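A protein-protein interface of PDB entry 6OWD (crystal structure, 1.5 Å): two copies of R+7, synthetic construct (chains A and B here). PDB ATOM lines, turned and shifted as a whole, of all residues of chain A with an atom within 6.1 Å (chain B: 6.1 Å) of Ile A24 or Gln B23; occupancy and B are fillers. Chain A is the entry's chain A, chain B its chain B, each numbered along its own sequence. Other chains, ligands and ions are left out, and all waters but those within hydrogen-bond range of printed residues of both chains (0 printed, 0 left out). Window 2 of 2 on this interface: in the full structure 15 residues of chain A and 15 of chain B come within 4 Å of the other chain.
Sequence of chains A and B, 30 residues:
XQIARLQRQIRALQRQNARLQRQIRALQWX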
ATOM      1  N   ARG A  19     -14.974 -19.094 -22.920  1.00  0.00           N
ATOM      2  CA  ARG A  19     -14.281 -20.252 -22.365  1.00  0.00           C
ATOM      3  C   ARG A  19     -13.378 -19.879 -21.189  1.00  0.00           C
ATOM      4  O   ARG A  19     -13.231 -20.643 -20.245  1.00  0.00           O
ATOM      5  CB  ARG A  19     -13.462 -20.929 -23.459  1.00  0.00           C
ATOM      6  CG  ARG A  19     -14.334 -21.873 -24.359  1.00  0.00           C
ATOM      7  CD  ARG A  19     -13.588 -22.235 -25.645  1.00  0.00           C
ATOM      8  NE  ARG A  19     -14.395 -23.169 -26.434  1.00  0.00           N
ATOM      9  CZ  ARG A  19     -14.161 -23.494 -27.701  1.00  0.00           C
ATOM     10  NH1 ARG A  19     -13.152 -22.919 -28.334  1.00  0.00           N
ATOM     11  NH2 ARG A  19     -14.935 -24.388 -28.333  1.00  0.00           N
ATOM     12  N   LEU A  20     -12.712 -18.747 -21.272  1.00  0.00           N
ATOM     13  CA  LEU A  20     -11.893 -18.274 -20.167  1.00  0.00           C
ATOM     14  C   LEU A  20     -12.738 -17.932 -18.948  1.00  0.00           C
ATOM     15  O   LEU A  20     -12.316 -18.204 -17.827  1.00  0.00           O
ATOM     16  CB  LEU A  20     -11.016 -17.089 -20.657  1.00  0.00           C
ATOM     17  CG  LEU A  20     -10.096 -17.504 -21.827  1.00  0.00           C
ATOM     18  CD1 LEU A  20      -9.334 -16.313 -22.309  1.00  0.00           C
ATOM     19  CD2 LEU A  20      -9.132 -18.629 -21.432  1.00  0.00           C
ATOM     20  N   GLN A  21     -13.861 -17.238 -19.118  1.00  0.00           N
ATOM     21  CA  GLN A  21     -14.675 -16.928 -17.956  1.00  0.00           C
ATOM     22  C   GLN A  21     -15.098 -18.195 -17.284  1.00  0.00           C
ATOM     23  O   GLN A  21     -15.190 -18.236 -16.062  1.00  0.00           O
ATOM     24  CB  GLN A  21     -15.913 -16.135 -18.377  1.00  0.00           C
ATOM     25  CG  GLN A  21     -15.617 -14.773 -18.855  1.00  0.00           C
ATOM     26  CD  GLN A  21     -16.900 -13.930 -19.047  1.00  0.00           C
ATOM     27  OE1 GLN A  21     -17.965 -14.256 -18.496  1.00  0.00           O
ATOM     28  NE2 GLN A  21     -16.786 -12.835 -19.777  1.00  0.00           N
ATOM     29  N   ARG A  22     -15.416 -19.223 -18.089  1.00  0.00           N
ATOM     30  CA  ARG A  22     -15.819 -20.511 -17.545  1.00  0.00           C
ATOM     31  C   ARG A  22     -14.710 -21.071 -16.689  1.00  0.00           C
ATOM     32  O   ARG A  22     -14.974 -21.646 -15.625  1.00  0.00           O
ATOM     33  CB  ARG A  22     -16.156 -21.463 -18.696  1.00  0.00           C
ATOM     34  CG  ARG A  22     -17.104 -22.572 -18.347  1.00  0.00           C
ATOM     35  CD  ARG A  22     -18.125 -22.823 -19.469  1.00  0.00           C
ATOM     36  NE  ARG A  22     -17.507 -22.940 -20.786  1.00  0.00           N
ATOM     37  CZ  ARG A  22     -17.936 -22.281 -21.869  1.00  0.00           C
ATOM     38  NH1 ARG A  22     -19.008 -21.440 -21.833  1.00  0.00           N
ATOM     39  NH2 ARG A  22     -17.298 -22.470 -23.007  1.00  0.00           N
ATOM     40  N   GLN A  23     -13.478 -20.961 -17.183  1.00  0.00           N
ATOM     41  CA  GLN A  23     -12.335 -21.507 -16.469  1.00  0.00           C
ATOM     42  C   GLN A  23     -12.158 -20.761 -15.175  1.00  0.00           C
ATOM     43  O   GLN A  23     -11.825 -21.345 -14.154  1.00  0.00           O
ATOM     44  CB  GLN A  23     -11.085 -21.372 -17.350  1.00  0.00           C
ATOM     45  CG  GLN A  23     -10.759 -22.503 -18.273  1.00  0.00           C
ATOM     46  CD  GLN A  23      -9.403 -22.279 -18.988  1.00  0.00           C
ATOM     47  OE1 GLN A  23      -9.369 -21.953 -20.150  1.00  0.00           O
ATOM     48  NE2 GLN A  23      -8.305 -22.476 -18.268  1.00  0.00           N
ATOM     49  N   ILE A  24     -12.272 -19.432 -15.225  1.00  0.00           N
ATOM     50  CA  ILE A  24     -12.050 -18.695 -13.988  1.00  0.00           C
ATOM     51  C   ILE A  24     -13.078 -19.085 -12.953  1.00  0.00           C
ATOM     52  O   ILE A  24     -12.758 -19.294 -11.776  1.00  0.00           O
ATOM     53  CB  ILE A  24     -12.070 -17.196 -14.280  1.00  0.00           C
ATOM     54  CG1 ILE A  24     -10.857 -16.878 -15.128  1.00  0.00           C
ATOM     55  CG2 ILE A  24     -11.984 -16.358 -12.955  1.00  0.00           C
ATOM     56  CD1 ILE A  24     -10.684 -15.426 -15.476  1.00  0.00           C
ATOM     57  N   ARG A  25     -14.346 -19.193 -13.354  1.00  0.00           N
ATOM     58  CA  ARG A  25     -15.393 -19.577 -12.417  1.00  0.00           C
ATOM     59  C   ARG A  25     -15.117 -20.942 -11.810  1.00  0.00           C
ATOM     60  O   ARG A  25     -15.283 -21.140 -10.602  1.00  0.00           O
ATOM     61  CB  ARG A  25     -16.736 -19.582 -13.134  1.00  0.00           C
ATOM     62  CG  ARG A  25     -17.932 -19.897 -12.242  1.00  0.00           C
ATOM     63  CD  ARG A  25     -19.244 -19.767 -13.021  1.00  0.00           C
ATOM     64  NE  ARG A  25     -19.623 -18.370 -13.245  1.00  0.00           N
ATOM     65  CZ  ARG A  25     -19.663 -17.768 -14.431  1.00  0.00           C
ATOM     66  NH1 ARG A  25     -19.340 -18.415 -15.559  1.00  0.00           N
ATOM     67  NH2 ARG A  25     -20.041 -16.502 -14.481  1.00  0.00           N
ATOM     68  N   ALA A  26     -14.668 -21.895 -12.626  1.00  0.00           N
ATOM     69  CA  ALA A  26     -14.305 -23.211 -12.092  1.00  0.00           C
ATOM     70  C   ALA A  26     -13.141 -23.166 -11.111  1.00  0.00           C
ATOM     71  O   ALA A  26     -13.109 -23.952 -10.155  1.00  0.00           O
ATOM     72  CB  ALA A  26     -13.997 -24.176 -13.260  1.00  0.00           C
ATOM     73  N   LEU A  27     -12.142 -22.332 -11.381  1.00  0.00           N
ATOM     74  CA  LEU A  27     -10.956 -22.269 -10.544  1.00  0.00           C
ATOM     75  C   LEU A  27     -11.182 -21.526  -9.240  1.00  0.00           C
ATOM     76  O   LEU A  27     -10.496 -21.811  -8.250  1.00  0.00           O
ATOM     77  CB  LEU A  27      -9.839 -21.592 -11.314  1.00  0.00           C
ATOM     78  CG  LEU A  27      -9.117 -22.495 -12.331  1.00  0.00           C
ATOM     79  CD1 LEU A  27      -8.494 -21.696 -13.444  1.00  0.00           C
ATOM     80  CD2 LEU A  27      -7.957 -23.346 -11.643  1.00  0.00           C
ATOM     81  N   GLN A  28     -12.055 -20.538  -9.233  1.00  0.00           N
ATOM     82  CA  GLN A  28     -12.269 -19.748  -8.025  1.00  0.00           C
ATOM     83  C   GLN A  28     -12.913 -20.630  -6.957  1.00  0.00           C
ATOM     84  O   GLN A  28     -13.763 -21.479  -7.257  1.00  0.00           O
ATOM     85  CB  GLN A  28     -13.116 -18.511  -8.370  1.00  0.00           C
ATOM     86  CG  GLN A  28     -12.359 -17.409  -9.108  1.00  0.00           C
ATOM     87  CD  GLN A  28     -13.215 -16.119  -9.308  1.00  0.00           C
ATOM     88  OE1 GLN A  28     -14.436 -16.117  -9.124  1.00  0.00           O
ATOM     89  NE2 GLN A  28     -12.560 -15.020  -9.701  1.00  0.00           N
ATOM     90  N   ALA B  18      -6.438 -11.366 -22.541  1.00  0.00           N
ATOM     91  CA  ALA B  18      -5.123 -11.442 -21.873  1.00  0.00           C
ATOM     92  C   ALA B  18      -5.259 -11.223 -20.378  1.00  0.00           C
ATOM     93  O   ALA B  18      -4.664 -11.959 -19.582  1.00  0.00           O
ATOM     94  CB  ALA B  18      -4.174 -10.426 -22.478  1.00  0.00           C
ATOM     95  N   ARG B  19      -6.176 -10.330 -19.985  1.00  0.00           N
ATOM     96  CA  ARG B  19      -6.501 -10.098 -18.579  1.00  0.00           C
ATOM     97  C   ARG B  19      -7.086 -11.319 -17.921  1.00  0.00           C
ATOM     98  O   ARG B  19      -6.624 -11.747 -16.863  1.00  0.00           O
ATOM     99  CB  ARG B  19      -7.498  -8.980 -18.499  1.00  0.00           C
ATOM    100  CG  ARG B  19      -7.623  -8.277 -17.219  1.00  0.00           C
ATOM    101  CD  ARG B  19      -8.559  -7.050 -17.372  1.00  0.00           C
ATOM    102  NE  ARG B  19      -8.933  -6.494 -16.080  1.00  0.00           N
ATOM    103  CZ  ARG B  19      -8.128  -5.767 -15.347  1.00  0.00           C
ATOM    104  NH1 ARG B  19      -6.910  -5.492 -15.781  1.00  0.00           N
ATOM    105  NH2 ARG B  19      -8.558  -5.276 -14.214  1.00  0.00           N
ATOM    106  N   LEU B  20      -8.030 -11.970 -18.591  1.00  0.00           N
ATOM    107  CA  LEU B  20      -8.552 -13.188 -18.030  1.00  0.00           C
ATOM    108  C   LEU B  20      -7.480 -14.269 -17.936  1.00  0.00           C
ATOM    109  O   LEU B  20      -7.470 -15.025 -16.963  1.00  0.00           O
ATOM    110  CB  LEU B  20      -9.708 -13.640 -18.880  1.00  0.00           C
ATOM    111  CG  LEU B  20     -10.984 -12.842 -18.749  1.00  0.00           C
ATOM    112  CD1 LEU B  20     -12.032 -13.337 -19.822  1.00  0.00           C
ATOM    113  CD2 LEU B  20     -11.596 -12.880 -17.446  1.00  0.00           C
ATOM    114  N   GLN B  21      -6.683 -14.449 -18.999  1.00  0.00           N
ATOM    115  CA  GLN B  21      -5.629 -15.470 -19.020  1.00  0.00           C
ATOM    116  C   GLN B  21      -4.614 -15.238 -17.909  1.00  0.00           C
ATOM    117  O   GLN B  21      -4.102 -16.208 -17.345  1.00  0.00           O
ATOM    118  CB  GLN B  21      -4.912 -15.490 -20.367  1.00  0.00           C
ATOM    119  CG  GLN B  21      -3.914 -16.675 -20.493  1.00  0.00           C
ATOM    120  CD  GLN B  21      -4.551 -18.031 -20.590  1.00  0.00           C
ATOM    121  OE1 GLN B  21      -4.188 -18.992 -19.862  1.00  0.00           O
ATOM    122  NE2 GLN B  21      -5.445 -18.149 -21.502  1.00  0.00           N
ATOM    123  N   ARG B  22      -4.279 -13.966 -17.587  1.00  0.00           N
ATOM    124  CA  ARG B  22      -3.414 -13.698 -16.426  1.00  0.00           C
ATOM    125  C   ARG B  22      -4.038 -14.200 -15.117  1.00  0.00           C
ATOM    126  O   ARG B  22      -3.328 -14.680 -14.220  1.00  0.00           O
ATOM    127  CB  ARG B  22      -3.131 -12.194 -16.295  1.00  0.00           C
ATOM    128  CG  ARG B  22      -2.057 -11.729 -17.178  1.00  0.00           C
ATOM    129  CD  ARG B  22      -1.375 -10.550 -16.560  1.00  0.00           C
ATOM    130  NE  ARG B  22      -2.299  -9.507 -16.245  1.00  0.00           N
ATOM    131  CZ  ARG B  22      -2.829  -8.662 -17.117  1.00  0.00           C
ATOM    132  NH1 ARG B  22      -2.564  -8.751 -18.431  1.00  0.00           N
ATOM    133  NH2 ARG B  22      -3.632  -7.721 -16.655  1.00  0.00           N
ATOM    134  N   GLN B  23      -5.351 -14.022 -14.962  1.00  0.00           N
ATOM    135  CA  GLN B  23      -6.031 -14.478 -13.767  1.00  0.00           C
ATOM    136  C   GLN B  23      -6.051 -15.976 -13.721  1.00  0.00           C
ATOM    137  O   GLN B  23      -5.815 -16.561 -12.677  1.00  0.00           O
ATOM    138  CB  GLN B  23      -7.448 -13.988 -13.717  1.00  0.00           C
ATOM    139  CG  GLN B  23      -7.576 -12.470 -13.659  1.00  0.00           C
ATOM    140  CD  GLN B  23      -9.061 -12.035 -13.765  1.00  0.00           C
ATOM    141  OE1 GLN B  23      -9.438 -11.281 -14.680  1.00  0.00           O
ATOM    142  NE2 GLN B  23      -9.886 -12.501 -12.846  1.00  0.00           N
ATOM    143  N   ILE B  24      -6.258 -16.609 -14.865  1.00  0.00           N
ATOM    144  CA  ILE B  24      -6.250 -18.059 -14.893  1.00  0.00           C
ATOM    145  C   ILE B  24      -4.879 -18.577 -14.470  1.00  0.00           C
ATOM    146  O   ILE B  24      -4.769 -19.537 -13.706  1.00  0.00           O
ATOM    147  CB  ILE B  24      -6.666 -18.576 -16.280  1.00  0.00           C
ATOM    148  CG1 ILE B  24      -8.175 -18.334 -16.458  1.00  0.00           C
ATOM    149  CG2 ILE B  24      -6.252 -20.042 -16.492  1.00  0.00           C
ATOM    150  CD1 ILE B  24      -8.585 -18.339 -17.881  1.00  0.00           C
ATOM    151  N   ARG B  25      -3.819 -17.996 -15.030  1.00  0.00           N
ATOM    152  CA  ARG B  25      -2.473 -18.421 -14.685  1.00  0.00           C
ATOM    153  C   ARG B  25      -2.224 -18.315 -13.193  1.00  0.00           C
ATOM    154  O   ARG B  25      -1.653 -19.227 -12.577  1.00  0.00           O
ATOM    155  CB  ARG B  25      -1.471 -17.572 -15.446  1.00  0.00           C
ATOM    156  CG  ARG B  25      -1.346 -17.906 -16.906  1.00  0.00           C
ATOM    157  CD  ARG B  25      -0.075 -17.474 -17.514  1.00  0.00           C
ATOM    158  NE  ARG B  25       0.067 -16.046 -17.518  1.00  0.00           N
ATOM    159  CZ  ARG B  25      -0.260 -15.258 -18.534  1.00  0.00           C
ATOM    160  NH1 ARG B  25      -0.692 -15.738 -19.697  1.00  0.00           N
ATOM    161  NH2 ARG B  25      -0.052 -13.957 -18.423  1.00  0.00           N
ATOM    162  N   ALA B  26      -2.736 -17.262 -12.574  1.00  0.00           N
ATOM    163  CA  ALA B  26      -2.580 -17.081 -11.134  1.00  0.00           C
ATOM    164  C   ALA B  26      -3.286 -18.170 -10.321  1.00  0.00           C
ATOM    165  O   ALA B  26      -2.890 -18.467  -9.212  1.00  0.00           O
ATOM    166  CB  ALA B  26      -3.129 -15.706 -10.756  1.00  0.00           C
ATOM    167  N   LEU B  27      -4.360 -18.738 -10.826  1.00  0.00           N
ATOM    168  CA  LEU B  27      -5.188 -19.680 -10.085  1.00  0.00           C
ATOM    169  C   LEU B  27      -4.784 -21.126 -10.313  1.00  0.00           C
ATOM    170  O   LEU B  27      -5.228 -22.008  -9.577  1.00  0.00           O
ATOM    171  CB  LEU B  27      -6.626 -19.468 -10.510  1.00  0.00           C
ATOM    172  CG  LEU B  27      -7.296 -18.187 -10.027  1.00  0.00           C
ATOM    173  CD1 LEU B  27      -8.649 -17.964 -10.737  1.00  0.00           C
ATOM    174  CD2 LEU B  27      -7.458 -18.202  -8.545  1.00  0.00           C
ATOM    175  N   GLN B  28      -3.975 -21.369 -11.327  1.00  0.00           N
ATOM    176  CA  GLN B  28      -3.491 -22.705 -11.631  1.00  0.00           C
ATOM    177  C   GLN B  28      -2.446 -23.149 -10.602  1.00  0.00           C
ATOM    178  O   GLN B  28      -1.848 -22.362  -9.873  1.00  0.00           O
ATOM    179  CB  GLN B  28      -2.935 -22.763 -13.025  1.00  0.00           C
ATOM    180  CG  GLN B  28      -4.073 -22.763 -14.113  1.00  0.00           C
ATOM    181  CD  GLN B  28      -3.572 -22.547 -15.501  1.00  0.00           C
ATOM    182  OE1 GLN B  28      -2.563 -21.893 -15.728  1.00  0.00           O
ATOM    183  NE2 GLN B  28      -4.311 -23.068 -16.460  1.00  0.00           N
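Among the printed residues, merely in contact across the chains: Ile A24 with Ile B24, Ile A24 with Leu B20, Leu A20 with Ile B24, Gln A23 with Ile B24, Leu A27 with Leu B27, Leu A20 with Gln B21, Ile A24 with Gln B23, Leu A20 with Leu B20 and Gln A21 with Leu B20.
Ile A24 touches just these residues of chain B: Leu B20 (3.3 Å), Gln B23 (3.95 Å) and Ile B24 (3.3 Å).
Of chain A, only Ile A24 (3.95 Å) comes within 4 Å of Gln B23.
Printed residues of chain B within 4 Å of Gln A21: Leu B20.
Of the printed residues of chain B, Leu A20 touches Leu B20 (3.98 Å), Gln B21 (3.7 Å) and Ile B24 (3.6 Å).
Printed residues of chain B within 4 Å of Gln A23: Ile B24.
Arg A25 touches none of the printed residues of chain B.
Gln B28 touches none of the printed residues of chain A.
The nearest residue of chain A that does not touch Gln B23 is Gln A28 (4.8 Å).
The nearest printed residue of chain A that does not touch Leu B27 is Gln A28 (4.1 Å).
Of the 11 printed residues of chain B, 5 touch a printed residue of chain A.
Printed residues of chain B that touch a printed residue of chain A: Leu B20, Gln B21, Gln B23, Ile B24 and Leu B27.
Hydrophobic or aromatic side chains of chain B within 4 Å of the printed part of chain A: Leu B20, Ile B24 and Leu B27.
Among the printed residues, no Asp or Glu carboxylate lies within 4 Å of a Lys or Arg side-chain nitrogen of the other chain.
Leu A20 touches its own counterpart, Leu B20.
Leu A20 touches Ile B24, and with the chains exchanged Ile A24 touches Leu B20.
Ile A24 touches its own counterpart, Ile B24.
Leu A27 touches its own counterpart, Leu B27.
Of the 9 pairs that touch across the chains among the printed residues, 9 have their exchanged pair printed and touching as well.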
